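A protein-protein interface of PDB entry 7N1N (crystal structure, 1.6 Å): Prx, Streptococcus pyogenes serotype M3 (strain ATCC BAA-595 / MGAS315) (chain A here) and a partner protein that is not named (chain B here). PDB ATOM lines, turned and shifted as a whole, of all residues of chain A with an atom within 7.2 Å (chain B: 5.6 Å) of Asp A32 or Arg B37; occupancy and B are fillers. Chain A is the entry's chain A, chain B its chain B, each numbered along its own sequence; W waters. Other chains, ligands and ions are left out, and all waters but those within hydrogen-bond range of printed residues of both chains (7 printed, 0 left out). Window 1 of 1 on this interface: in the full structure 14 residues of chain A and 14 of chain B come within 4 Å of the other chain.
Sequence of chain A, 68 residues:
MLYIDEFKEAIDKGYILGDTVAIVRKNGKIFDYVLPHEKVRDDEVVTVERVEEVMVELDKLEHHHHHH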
ATOM      1  N   MET A   1      -6.645 -10.645  16.366  1.00  0.00           N
ATOM      2  CA  MET A   1      -5.462  -9.831  16.725  1.00  0.00           C
ATOM      3  C   MET A   1      -4.895  -9.096  15.516  1.00  0.00           C
ATOM      4  O   MET A   1      -4.565  -9.712  14.499  1.00  0.00           O
ATOM      5  CB  MET A   1      -4.387 -10.715  17.330  1.00  0.00           C
ATOM      6  CG  MET A   1      -3.697 -10.036  18.482  1.00  0.00           C
ATOM      7  SD  MET A   1      -2.160 -10.814  18.880  1.00  0.00           S
ATOM      8  CE  MET A   1      -2.738 -12.265  19.771  1.00  0.00           C
ATOM      9  N   LEU A   2      -4.773  -7.778  15.634  1.00  0.00           N
ATOM     10  CA  LEU A   2      -4.352  -6.925  14.529  1.00  0.00           C
ATOM     11  C   LEU A   2      -3.500  -5.785  15.059  1.00  0.00           C
ATOM     12  O   LEU A   2      -3.910  -5.081  15.987  1.00  0.00           O
ATOM     13  CB  LEU A   2      -5.561  -6.358  13.774  1.00  0.00           C
ATOM     14  CG  LEU A   2      -5.293  -5.418  12.596  1.00  0.00           C
ATOM     15  CD1 LEU A   2      -4.623  -6.213  11.458  1.00  0.00           C
ATOM     16  CD2 LEU A   2      -6.552  -4.717  12.120  1.00  0.00           C
ATOM     17  N   PHE A   7      -1.966  -3.618   9.306  1.00  0.00           N
ATOM     18  CA  PHE A   7      -2.977  -2.733   8.735  1.00  0.00           C
ATOM     19  C   PHE A   7      -2.355  -1.790   7.713  1.00  0.00           C
ATOM     20  O   PHE A   7      -2.903  -1.596   6.619  1.00  0.00           O
ATOM     21  CB  PHE A   7      -3.665  -1.967   9.883  1.00  0.00           C
ATOM     22  CG  PHE A   7      -4.902  -1.221   9.475  1.00  0.00           C
ATOM     23  CD1 PHE A   7      -6.015  -1.899   9.025  1.00  0.00           C
ATOM     24  CD2 PHE A   7      -4.957   0.160   9.577  1.00  0.00           C
ATOM     25  CE1 PHE A   7      -7.158  -1.219   8.657  1.00  0.00           C
ATOM     26  CE2 PHE A   7      -6.094   0.846   9.203  1.00  0.00           C
ATOM     27  CZ  PHE A   7      -7.198   0.145   8.735  1.00  0.00           C
ATOM     28  N   ALA A  10      -1.711  -3.533   4.460  1.00  0.00           N
ATOM     29  CA  ALA A  10      -2.903  -3.702   3.637  1.00  0.00           C
ATOM     30  C   ALA A  10      -3.234  -2.419   2.883  1.00  0.00           C
ATOM     31  O   ALA A  10      -3.672  -2.465   1.732  1.00  0.00           O
ATOM     32  CB  ALA A  10      -4.086  -4.130   4.505  1.00  0.00           C
ATOM     33  N   LYS A  13      -0.259  -1.773   0.115  1.00  0.00           N
ATOM     34  CA  LYS A  13      -0.324  -2.697  -1.010  1.00  0.00           C
ATOM     35  C   LYS A  13      -1.613  -2.576  -1.807  1.00  0.00           C
ATOM     36  O   LYS A  13      -1.757  -3.265  -2.818  1.00  0.00           O
ATOM     37  CB  LYS A  13      -0.141  -4.128  -0.497  1.00  0.00           C
ATOM     38  CG  LYS A  13       1.262  -4.397   0.057  1.00  0.00           C
ATOM     39  CD  LYS A  13       1.413  -5.825   0.583  1.00  0.00           C
ATOM     40  CE  LYS A  13       1.606  -6.827  -0.532  1.00  0.00           C
ATOM     41  NZ  LYS A  13       1.788  -8.210   0.027  1.00  0.00           N
ATOM     42  N   TYR A  15      -4.805  -3.256  -0.817  1.00  0.00           N
ATOM     43  CA  TYR A  15      -5.942  -4.093  -0.458  1.00  0.00           C
ATOM     44  C   TYR A  15      -7.050  -3.306   0.235  1.00  0.00           C
ATOM     45  O   TYR A  15      -8.226  -3.689   0.141  1.00  0.00           O
ATOM     46  CB  TYR A  15      -5.475  -5.238   0.432  1.00  0.00           C
ATOM     47  CG  TYR A  15      -4.590  -6.245  -0.268  1.00  0.00           C
ATOM     48  CD1 TYR A  15      -5.136  -7.263  -1.034  1.00  0.00           C
ATOM     49  CD2 TYR A  15      -3.209  -6.193  -0.140  1.00  0.00           C
ATOM     50  CE1 TYR A  15      -4.344  -8.193  -1.656  1.00  0.00           C
ATOM     51  CE2 TYR A  15      -2.406  -7.121  -0.764  1.00  0.00           C
ATOM     52  CZ  TYR A  15      -2.972  -8.117  -1.533  1.00  0.00           C
ATOM     53  OH  TYR A  15      -2.184  -9.059  -2.167  1.00  0.00           O
ATOM     54  N   ALA A  22     -14.203  -2.183   6.820  1.00  0.00           N
ATOM     55  CA  ALA A  22     -14.946  -3.003   7.764  1.00  0.00           C
ATOM     56  C   ALA A  22     -13.991  -3.551   8.814  1.00  0.00           C
ATOM     57  O   ALA A  22     -12.925  -4.084   8.475  1.00  0.00           O
ATOM     58  CB  ALA A  22     -15.653  -4.147   7.038  1.00  0.00           C
ATOM     59  N   ILE A  23     -14.380  -3.427  10.082  1.00  0.00           N
ATOM     60  CA  ILE A  23     -13.553  -3.811  11.219  1.00  0.00           C
ATOM     61  C   ILE A  23     -14.347  -4.770  12.095  1.00  0.00           C
ATOM     62  O   ILE A  23     -15.516  -4.508  12.403  1.00  0.00           O
ATOM     63  CB  ILE A  23     -13.124  -2.585  12.049  1.00  0.00           C
ATOM     64  CG1 ILE A  23     -12.188  -1.675  11.248  1.00  0.00           C
ATOM     65  CG2 ILE A  23     -12.469  -3.027  13.356  1.00  0.00           C
ATOM     66  CD1 ILE A  23     -10.858  -2.303  10.944  1.00  0.00           C
ATOM     67  N   VAL A  24     -13.709  -5.863  12.508  1.00  0.00           N
ATOM     68  CA  VAL A  24     -14.246  -6.745  13.535  1.00  0.00           C
ATOM     69  C   VAL A  24     -13.625  -6.334  14.862  1.00  0.00           C
ATOM     70  O   VAL A  24     -12.396  -6.223  14.975  1.00  0.00           O
ATOM     71  CB  VAL A  24     -13.953  -8.225  13.243  1.00  0.00           C
ATOM     72  CG1 VAL A  24     -14.352  -9.073  14.466  1.00  0.00           C
ATOM     73  CG2 VAL A  24     -14.697  -8.684  12.008  1.00  0.00           C
ATOM     74  N   ARG A  25     -14.469  -6.076  15.851  1.00  0.00           N
ATOM     75  CA  ARG A  25     -14.038  -5.884  17.228  1.00  0.00           C
ATOM     76  C   ARG A  25     -14.453  -7.097  18.042  1.00  0.00           C
ATOM     77  O   ARG A  25     -15.584  -7.579  17.917  1.00  0.00           O
ATOM     78  CB  ARG A  25     -14.641  -4.612  17.815  1.00  0.00           C
ATOM     79  CG  ARG A  25     -13.963  -3.357  17.294  1.00  0.00           C
ATOM     80  CD  ARG A  25     -14.586  -2.091  17.833  1.00  0.00           C
ATOM     81  NE  ARG A  25     -13.988  -0.916  17.218  1.00  0.00           N
ATOM     82  CZ  ARG A  25     -12.982  -0.232  17.746  1.00  0.00           C
ATOM     83  NH1 ARG A  25     -12.481  -0.545  18.927  1.00  0.00           N
ATOM     84  NH2 ARG A  25     -12.459   0.781  17.065  1.00  0.00           N
ATOM     85  N   LYS A  26     -13.534  -7.592  18.863  1.00  0.00           N
ATOM     86  CA  LYS A  26     -13.796  -8.702  19.769  1.00  0.00           C
ATOM     87  C   LYS A  26     -13.403  -8.234  21.160  1.00  0.00           C
ATOM     88  O   LYS A  26     -12.318  -7.673  21.345  1.00  0.00           O
ATOM     89  CB  LYS A  26     -13.027  -9.961  19.370  1.00  0.00           C
ATOM     90  CG  LYS A  26     -13.516 -11.204  20.094  1.00  0.00           C
ATOM     91  CD  LYS A  26     -12.869 -12.467  19.540  1.00  0.00           C
ATOM     92  CE  LYS A  26     -13.358 -12.775  18.132  1.00  0.00           C
ATOM     93  NZ  LYS A  26     -13.115 -14.209  17.777  1.00  0.00           N
ATOM     94  N   LYS A  29     -12.271  -4.564  21.247  1.00  0.00           N
ATOM     95  CA  LYS A  29     -11.021  -4.090  20.674  1.00  0.00           C
ATOM     96  C   LYS A  29     -10.826  -4.595  19.251  1.00  0.00           C
ATOM     97  O   LYS A  29     -11.362  -5.633  18.864  1.00  0.00           O
ATOM     98  CB  LYS A  29      -9.829  -4.523  21.536  1.00  0.00           C
ATOM     99  CG  LYS A  29      -9.791  -3.836  22.886  1.00  0.00           C
ATOM    100  CD  LYS A  29      -8.478  -4.064  23.619  1.00  0.00           C
ATOM    101  CE  LYS A  29      -8.431  -3.230  24.901  1.00  0.00           C
ATOM    102  NZ  LYS A  29      -7.114  -3.315  25.600  1.00  0.00           N
ATOM    103  N   ILE A  30     -10.049  -3.834  18.475  1.00  0.00           N
ATOM    104  CA  ILE A  30      -9.860  -4.137  17.065  1.00  0.00           C
ATOM    105  C   ILE A  30      -9.208  -5.503  16.933  1.00  0.00           C
ATOM    106  O   ILE A  30      -8.104  -5.740  17.438  1.00  0.00           O
ATOM    107  CB  ILE A  30      -9.038  -3.038  16.375  1.00  0.00           C
ATOM    108  CG1 ILE A  30      -9.787  -1.711  16.444  1.00  0.00           C
ATOM    109  CG2 ILE A  30      -8.734  -3.433  14.939  1.00  0.00           C
ATOM    110  CD1 ILE A  30      -8.981  -0.518  15.968  1.00  0.00           C
ATOM    111  N   PHE A  31      -9.887  -6.405  16.236  1.00  0.00           N
ATOM    112  CA  PHE A  31      -9.505  -7.804  16.107  1.00  0.00           C
ATOM    113  C   PHE A  31      -9.017  -8.144  14.711  1.00  0.00           C
ATOM    114  O   PHE A  31      -8.044  -8.888  14.572  1.00  0.00           O
ATOM    115  CB  PHE A  31     -10.713  -8.680  16.490  1.00  0.00           C
ATOM    116  CG  PHE A  31     -10.524 -10.144  16.236  1.00  0.00           C
ATOM    117  CD1 PHE A  31      -9.791 -10.934  17.112  1.00  0.00           C
ATOM    118  CD2 PHE A  31     -11.095 -10.734  15.126  1.00  0.00           C
ATOM    119  CE1 PHE A  31      -9.619 -12.282  16.870  1.00  0.00           C
ATOM    120  CE2 PHE A  31     -10.919 -12.088  14.882  1.00  0.00           C
ATOM    121  CZ  PHE A  31     -10.187 -12.857  15.751  1.00  0.00           C
ATOM    122  N   ASP A  32      -9.634  -7.571  13.682  1.00  0.00           N
ATOM    123  CA  ASP A  32      -9.371  -7.908  12.283  1.00  0.00           C
ATOM    124  C   ASP A  32     -10.059  -6.860  11.422  1.00  0.00           C
ATOM    125  O   ASP A  32     -10.927  -6.121  11.889  1.00  0.00           O
ATOM    126  CB  ASP A  32      -9.899  -9.318  11.956  1.00  0.00           C
ATOM    127  CG  ASP A  32      -9.234  -9.970  10.758  1.00  0.00           C
ATOM    128  OD1 ASP A  32      -8.329  -9.382  10.145  1.00  0.00           O
ATOM    129  OD2 ASP A  32      -9.641 -11.113  10.424  1.00  0.00           O
ATOM    130  N   TYR A  33      -9.656  -6.795  10.165  1.00  0.00           N
ATOM    131  CA  TYR A  33     -10.425  -6.095   9.143  1.00  0.00           C
ATOM    132  C   TYR A  33     -11.101  -7.124   8.241  1.00  0.00           C
ATOM    133  O   TYR A  33     -10.787  -8.319   8.265  1.00  0.00           O
ATOM    134  CB  TYR A  33      -9.547  -5.123   8.338  1.00  0.00           C
ATOM    135  CG  TYR A  33      -8.311  -5.699   7.703  1.00  0.00           C
ATOM    136  CD1 TYR A  33      -7.124  -5.765   8.404  1.00  0.00           C
ATOM    137  CD2 TYR A  33      -8.324  -6.152   6.394  1.00  0.00           C
ATOM    138  CE1 TYR A  33      -5.973  -6.297   7.829  1.00  0.00           C
ATOM    139  CE2 TYR A  33      -7.179  -6.678   5.808  1.00  0.00           C
ATOM    140  CZ  TYR A  33      -6.007  -6.743   6.528  1.00  0.00           C
ATOM    141  OH  TYR A  33      -4.862  -7.254   5.949  1.00  0.00           O
ATOM    142  N   VAL A  34     -12.070  -6.652   7.459  1.00  0.00           N
ATOM    143  CA  VAL A  34     -12.820  -7.498   6.542  1.00  0.00           C
ATOM    144  C   VAL A  34     -12.889  -6.821   5.179  1.00  0.00           C
ATOM    145  O   VAL A  34     -13.331  -5.676   5.069  1.00  0.00           O
ATOM    146  CB  VAL A  34     -14.240  -7.786   7.071  1.00  0.00           C
ATOM    147  CG1 VAL A  34     -14.963  -8.761   6.145  1.00  0.00           C
ATOM    148  CG2 VAL A  34     -14.171  -8.350   8.484  1.00  0.00           C
ATOM    149  N   LEU A  35     -12.456  -7.525   4.161  1.00  0.00           N
ATOM    150  CA  LEU A  35     -12.479  -7.063   2.788  1.00  0.00           C
ATOM    151  C   LEU A  35     -13.635  -7.702   2.038  1.00  0.00           C
ATOM    152  O   LEU A  35     -14.175  -8.732   2.458  1.00  0.00           O
ATOM    153  CB  LEU A  35     -11.157  -7.399   2.105  1.00  0.00           C
ATOM    154  CG  LEU A  35      -9.919  -6.848   2.816  1.00  0.00           C
ATOM    155  CD1 LEU A  35      -8.647  -7.214   2.065  1.00  0.00           C
ATOM    156  CD2 LEU A  35     -10.004  -5.343   3.010  1.00  0.00           C
ATOM    157  N   GLU A  38     -14.745 -11.612   1.850  1.00  0.00           N
ATOM    158  CA  GLU A  38     -14.275 -12.392   2.988  1.00  0.00           C
ATOM    159  C   GLU A  38     -15.443 -12.654   3.933  1.00  0.00           C
ATOM    160  O   GLU A  38     -16.337 -11.824   4.078  1.00  0.00           O
ATOM    161  CB  GLU A  38     -13.159 -11.663   3.734  1.00  0.00           C
ATOM    162  CG  GLU A  38     -11.909 -11.453   2.911  1.00  0.00           C
ATOM    163  CD  GLU A  38     -10.796 -10.792   3.698  1.00  0.00           C
ATOM    164  OE1 GLU A  38     -11.108  -9.998   4.589  1.00  0.00           O
ATOM    165  OE2 GLU A  38      -9.609 -11.061   3.443  1.00  0.00           O
ATOM    166  N   LYS A  39     -15.425 -13.811   4.588  1.00  0.00           N
ATOM    167  CA  LYS A  39     -16.551 -14.275   5.391  1.00  0.00           C
ATOM    168  C   LYS A  39     -16.481 -13.729   6.810  1.00  0.00           C
ATOM    169  O   LYS A  39     -15.403 -13.657   7.406  1.00  0.00           O
ATOM    170  CB  LYS A  39     -16.590 -15.809   5.427  1.00  0.00           C
ATOM    171  CG  LYS A  39     -16.338 -16.494   4.090  1.00  0.00           C
ATOM    172  CD  LYS A  39     -16.399 -18.024   4.205  1.00  0.00           C
ATOM    173  CE  LYS A  39     -15.566 -18.534   5.355  1.00  0.00           C
ATOM    174  NZ  LYS A  39     -15.532 -20.028   5.479  1.00  0.00           N
ATOM    175  N   GLU A  44     -19.429 -12.358  15.251  1.00  0.00           N
ATOM    176  CA  GLU A  44     -18.439 -11.292  15.130  1.00  0.00           C
ATOM    177  C   GLU A  44     -19.157  -9.950  15.006  1.00  0.00           C
ATOM    178  O   GLU A  44     -20.157  -9.829  14.295  1.00  0.00           O
ATOM    179  CB  GLU A  44     -17.519 -11.531  13.928  1.00  0.00           C
ATOM    180  CG  GLU A  44     -16.481 -12.628  14.164  1.00  0.00           C
ATOM    181  CD  GLU A  44     -15.586 -12.881  12.965  1.00  0.00           C
ATOM    182  OE1 GLU A  44     -16.101 -12.910  11.829  1.00  0.00           O
ATOM    183  OE2 GLU A  44     -14.362 -13.071  13.159  1.00  0.00           O
ATOM    184  N   VAL A  45     -18.651  -8.946  15.717  1.00  0.00           N
ATOM    185  CA  VAL A  45     -19.211  -7.600  15.670  1.00  0.00           C
ATOM    186  C   VAL A  45     -18.447  -6.814  14.611  1.00  0.00           C
ATOM    187  O   VAL A  45     -17.240  -6.589  14.753  1.00  0.00           O
ATOM    188  CB  VAL A  45     -19.125  -6.908  17.039  1.00  0.00           C
ATOM    189  CG1 VAL A  45     -19.616  -5.471  16.928  1.00  0.00           C
ATOM    190  CG2 VAL A  45     -19.917  -7.687  18.081  1.00  0.00           C
ATOM    191  N   THR A  47     -18.148  -3.360  12.083  1.00  0.00           N
ATOM    192  CA  THR A  47     -18.446  -1.940  11.979  1.00  0.00           C
ATOM    193  C   THR A  47     -17.581  -1.339  10.882  1.00  0.00           C
ATOM    194  O   THR A  47     -16.402  -1.672  10.766  1.00  0.00           O
ATOM    195  CB  THR A  47     -18.159  -1.217  13.297  1.00  0.00           C
ATOM    196  OG1 THR A  47     -16.788  -1.435  13.663  1.00  0.00           O
ATOM    197  CG2 THR A  47     -19.057  -1.736  14.387  1.00  0.00           C
ATOM    198  N   SER B  31      -6.991 -15.268  12.684  1.00  0.00           N
ATOM    199  CA  SER B  31      -8.290 -15.576  12.102  1.00  0.00           C
ATOM    200  C   SER B  31      -8.090 -16.318  10.784  1.00  0.00           C
ATOM    201  O   SER B  31      -7.045 -16.223  10.144  1.00  0.00           O
ATOM    202  CB  SER B  31      -9.115 -14.315  11.866  1.00  0.00           C
ATOM    203  OG  SER B  31      -8.604 -13.613  10.743  1.00  0.00           O
ATOM    204  N   THR B  32      -9.122 -17.058  10.371  1.00  0.00           N
ATOM    205  CA  THR B  32      -9.033 -17.759   9.093  1.00  0.00           C
ATOM    206  C   THR B  32      -8.858 -16.783   7.938  1.00  0.00           C
ATOM    207  O   THR B  32      -8.126 -17.079   6.983  1.00  0.00           O
ATOM    208  CB  THR B  32     -10.262 -18.644   8.881  1.00  0.00           C
ATOM    209  OG1 THR B  32     -11.458 -17.869   8.941  1.00  0.00           O
ATOM    210  CG2 THR B  32     -10.315 -19.741   9.954  1.00  0.00           C
ATOM    211  N   ARG B  33      -9.472 -15.600   8.024  1.00  0.00           N
ATOM    212  CA  ARG B  33      -9.202 -14.564   7.031  1.00  0.00           C
ATOM    213  C   ARG B  33      -7.715 -14.237   6.992  1.00  0.00           C
ATOM    214  O   ARG B  33      -7.102 -14.173   5.921  1.00  0.00           O
ATOM    215  CB  ARG B  33     -10.010 -13.310   7.344  1.00  0.00           C
ATOM    216  CG  ARG B  33     -11.496 -13.425   7.097  1.00  0.00           C
ATOM    217  CD  ARG B  33     -12.228 -12.136   7.482  1.00  0.00           C
ATOM    218  NE  ARG B  33     -12.012 -11.796   8.883  1.00  0.00           N
ATOM    219  CZ  ARG B  33     -12.834 -12.122   9.869  1.00  0.00           C
ATOM    220  NH1 ARG B  33     -14.026 -12.651   9.631  1.00  0.00           N
ATOM    221  NH2 ARG B  33     -12.450 -11.912  11.125  1.00  0.00           N
ATOM    222  N   GLN B  34      -7.119 -14.016   8.164  1.00  0.00           N
ATOM    223  CA  GLN B  34      -5.709 -13.657   8.240  1.00  0.00           C
ATOM    224  C   GLN B  34      -4.817 -14.767   7.699  1.00  0.00           C
ATOM    225  O   GLN B  34      -3.842 -14.496   6.994  1.00  0.00           O
ATOM    226  CB  GLN B  34      -5.355 -13.317   9.690  1.00  0.00           C
ATOM    227  CG  GLN B  34      -5.850 -11.949  10.114  1.00  0.00           C
ATOM    228  CD  GLN B  34      -5.838 -11.759  11.618  1.00  0.00           C
ATOM    229  OE1 GLN B  34      -5.692 -12.709  12.372  1.00  0.00           O
ATOM    230  NE2 GLN B  34      -5.995 -10.525  12.055  1.00  0.00           N
ATOM    231  N   LEU B  35      -5.133 -16.027   8.013  1.00  0.00           N
ATOM    232  CA  LEU B  35      -4.324 -17.121   7.481  1.00  0.00           C
ATOM    233  C   LEU B  35      -4.393 -17.168   5.959  1.00  0.00           C
ATOM    234  O   LEU B  35      -3.379 -17.386   5.284  1.00  0.00           O
ATOM    235  CB  LEU B  35      -4.774 -18.460   8.068  1.00  0.00           C
ATOM    236  CG  LEU B  35      -4.034 -19.690   7.551  1.00  0.00           C
ATOM    237  CD1 LEU B  35      -2.525 -19.544   7.793  1.00  0.00           C
ATOM    238  CD2 LEU B  35      -4.550 -20.954   8.197  1.00  0.00           C
ATOM    239  N   THR B  36      -5.591 -16.982   5.399  1.00  0.00           N
ATOM    240  CA  THR B  36      -5.734 -16.958   3.949  1.00  0.00           C
ATOM    241  C   THR B  36      -4.850 -15.882   3.335  1.00  0.00           C
ATOM    242  O   THR B  36      -4.200 -16.114   2.309  1.00  0.00           O
ATOM    243  CB  THR B  36      -7.206 -16.734   3.586  1.00  0.00           C
ATOM    244  OG1 THR B  36      -7.996 -17.785   4.157  1.00  0.00           O
ATOM    245  CG2 THR B  36      -7.391 -16.741   2.088  1.00  0.00           C
ATOM    246  N   ARG B  37      -4.784 -14.709   3.968  1.00  0.00           N
ATOM    247  CA  ARG B  37      -3.975 -13.622   3.433  1.00  0.00           C
ATOM    248  C   ARG B  37      -2.487 -13.961   3.501  1.00  0.00           C
ATOM    249  O   ARG B  37      -1.693 -13.536   2.652  1.00  0.00           O
ATOM    250  CB  ARG B  37      -4.261 -12.331   4.188  1.00  0.00           C
ATOM    251  CG  ARG B  37      -5.686 -11.842   4.105  1.00  0.00           C
ATOM    252  CD  ARG B  37      -5.901 -10.636   5.022  1.00  0.00           C
ATOM    253  NE  ARG B  37      -7.315 -10.375   5.265  1.00  0.00           N
ATOM    254  CZ  ARG B  37      -7.814 -10.024   6.442  1.00  0.00           C
ATOM    255  NH1 ARG B  37      -7.042  -9.897   7.508  1.00  0.00           N
ATOM    256  NH2 ARG B  37      -9.122  -9.827   6.560  1.00  0.00           N
ATOM    257  N   ILE B  38      -2.077 -14.685   4.545  1.00  0.00           N
ATOM    258  CA  ILE B  38      -0.676 -15.062   4.671  1.00  0.00           C
ATOM    259  C   ILE B  38      -0.308 -16.071   3.594  1.00  0.00           C
ATOM    260  O   ILE B  38       0.766 -15.988   2.981  1.00  0.00           O
ATOM    261  CB  ILE B  38      -0.382 -15.617   6.076  1.00  0.00           C
ATOM    262  CG1 ILE B  38      -0.500 -14.512   7.118  1.00  0.00           C
ATOM    263  CG2 ILE B  38       1.024 -16.226   6.109  1.00  0.00           C
ATOM    264  CD1 ILE B  38      -0.600 -15.030   8.551  1.00  0.00           C
ATOM    265  N   GLU B  39      -1.205 -17.025   3.321  1.00  0.00           N
ATOM    266  CA  GLU B  39      -0.880 -18.095   2.382  1.00  0.00           C
ATOM    267  C   GLU B  39      -0.723 -17.582   0.957  1.00  0.00           C
ATOM    268  O   GLU B  39       0.011 -18.185   0.164  1.00  0.00           O
ATOM    269  CB  GLU B  39      -1.961 -19.180   2.440  1.00  0.00           C
ATOM    270  CG  GLU B  39      -1.903 -19.962   3.726  1.00  0.00           C
ATOM    271  CD  GLU B  39      -2.816 -21.157   3.788  1.00  0.00           C
ATOM    272  OE1 GLU B  39      -3.741 -21.269   2.954  1.00  0.00           O
ATOM    273  OE2 GLU B  39      -2.605 -21.993   4.696  1.00  0.00           O
ATOM    274  N   SER B  40      -1.404 -16.494   0.610  1.00  0.00           N
ATOM    275  CA  SER B  40      -1.318 -15.923  -0.727  1.00  0.00           C
ATOM    276  C   SER B  40      -0.203 -14.894  -0.861  1.00  0.00           C
ATOM    277  O   SER B  40       0.077 -14.443  -1.976  1.00  0.00           O
ATOM    278  CB  SER B  40      -2.638 -15.247  -1.107  1.00  0.00           C
ATOM    279  OG  SER B  40      -2.846 -14.124  -0.274  1.00  0.00           O
ATOM    280  N   GLY B  41       0.420 -14.498   0.245  1.00  0.00           N
ATOM    281  CA  GLY B  41       1.386 -13.428   0.259  1.00  0.00           C
ATOM    282  C   GLY B  41       0.784 -12.051   0.413  1.00  0.00           C
ATOM    283  O   GLY B  41       1.533 -11.071   0.540  1.00  0.00           O
ATOM    284  N   GLN B  42      -0.546 -11.958   0.419  1.00  0.00           N
ATOM    285  CA  GLN B  42      -1.216 -10.679   0.637  1.00  0.00           C
ATOM    286  C   GLN B  42      -0.708 -10.005   1.902  1.00  0.00           C
ATOM    287  O   GLN B  42      -0.419  -8.803   1.901  1.00  0.00           O
ATOM    288  CB  GLN B  42      -2.731 -10.920   0.698  1.00  0.00           C
ATOM    289  CG  GLN B  42      -3.536  -9.797   1.287  1.00  0.00           C
ATOM    290  CD  GLN B  42      -5.037  -9.993   1.101  1.00  0.00           C
ATOM    291  OE1 GLN B  42      -5.485 -10.853   0.327  1.00  0.00           O
ATOM    292  NE2 GLN B  42      -5.814  -9.173   1.774  1.00  0.00           N
ATOM    293  N   SER B  43      -0.576 -10.765   2.984  1.00  0.00           N
ATOM    294  CA  SER B  43      -0.134 -10.248   4.267  1.00  0.00           C
ATOM    295  C   SER B  43       1.138 -10.961   4.697  1.00  0.00           C
ATOM    296  O   SER B  43       1.252 -12.182   4.550  1.00  0.00           O
ATOM    297  CB  SER B  43      -1.209 -10.444   5.353  1.00  0.00           C
ATOM    298  OG  SER B  43      -2.338  -9.618   5.137  1.00  0.00           O
HETATM  299  O   HOH W   1      -8.395 -10.626   0.967  1.00  0.00           O
HETATM  300  O   HOH W   2      -6.672 -12.886  15.123  1.00  0.00           O
HETATM  301  O   HOH W   3     -14.194 -15.993   8.089  1.00  0.00           O
HETATM  302  O   HOH W   4      -2.032  -6.715   3.046  1.00  0.00           O
HETATM  303  O   HOH W   5      -4.063  -9.703   7.666  1.00  0.00           O
HETATM  304  O   HOH W   6      -8.842 -13.673   3.538  1.00  0.00           O
HETATM  305  O   HOH W   7      -4.728  -7.217   3.351  1.00  0.00           O
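The backbone carbonyl oxygen (O) of Met A1 is in hydrogen-bond range of the side-chain amide nitrogen (NE2) of Gln B34.
NZ of Lys A13 sits at hydrogen-bond distance from O of Gly B41, at 2.9 Å.
O of Gln B42 lies within hydrogen-bond range of NZ of Lys A13.
OD2 of Asp A32 lies within hydrogen-bond range of OG of Ser B31, 2.7 Å away.
The side-chain carboxylate of Asp A32 lies within salt-bridge range of the guanidinium group of Arg B33 (2.9 Å).
The side-chain amide nitrogen (NE2) of Gln B34 sits at hydrogen-bond distance from the side-chain carboxylate (OD1) of Asp A32 (3.2 Å).
The side-chain carboxylate of Asp A32 is in salt-bridge range of the guanidinium group of Arg B37 (3.0 Å).
The guanidinium group of Arg B37 sits at hydrogen-bond distance from the backbone carbonyl oxygen of Tyr A33 (2.8 Å).
The guanidinium group (NH2) of Arg B37 lies within salt-bridge range of the side-chain carboxylate (OE1) of Glu A38, at 2.8 Å.
The backbone carbonyl oxygen (O) of Lys A39 sits at hydrogen-bond distance from the guanidinium group (NH1) of Arg B33, 2.8 Å away.
The side-chain carboxylate (OE2) of Glu A44 is in salt-bridge range of the guanidinium group (NH2) of Arg B33 (3.0 Å).
Water W3 lies within hydrogen-bond range of O of Lys A39 and OG1 of Thr B32.
Water W6 lies within hydrogen-bond range of OE2 of Glu A38 and O of Arg B33.
Water W1 bridges the side-chain carboxylate (OE2) of Glu A38 (2.8 Å) and the side-chain amide oxygen (OE1) of Gln B42 (3.0 Å).
Ile A23 touches none of the printed residues of chain B.
Arg A25 touches none of the printed residues of chain B.
Asp A32 touches just these residues of chain B: Ser B31 (2.7 Å), Arg B33 (2.9 Å), Gln B34 (3.2 Å) and Arg B37 (3.0 Å).
Of the printed residues of chain B, Tyr A33 touches Arg B33, Arg B37 and Ser B43.
Of the printed residues of chain A, Ser B31 touches Asp A32.
Printed residues of chain A within 4 Å of Arg B33: Asp A32, Tyr A33, Glu A38, Lys A39 and Glu A44.
Of chain A, only Asp A32, Tyr A33 and Glu A38 come within 4 Å of Arg B37.
The nearest printed residue of chain B that does not touch Asp A32 is Thr B32 (6.0 Å).
The nearest printed residue of chain A that does not touch Arg B33 is Val A24 (4.03 Å).
Among the printed residues, pairs that only touch across the chains: Tyr A15 with Gln B42, Phe A31 with Gln B34, Tyr A33 with Arg B33, Tyr A33 with Ser B43, Leu A35 with Gln B42 and Glu A38 with Arg B33.
N of Val A24 lies within hydrogen-bond range of O of Asp A32, at 2.9 Å.
N of Leu A35 lies within hydrogen-bond range of OE1 of Glu A38.
OG of Ser B31 lies close to N of Arg B33 (3.5 Å).
The backbone carbonyl oxygen (O) of Arg B37 lies within hydrogen-bond range of the side-chain hydroxyl (OG) of Ser B40 (3.2 Å).
Hydrophobic or aromatic side chains of chain A within 4 Å of the printed part of chain B: Tyr A15, Tyr A33 and Leu A35.
Among the printed residues, Asp or Glu carboxylates within 4 Å of a Lys or Arg side-chain nitrogen of the other chain: Asp A32 with Arg B33, Asp A32 with Arg B37, Glu A38 with Arg B37 and Glu A44 with Arg B33.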
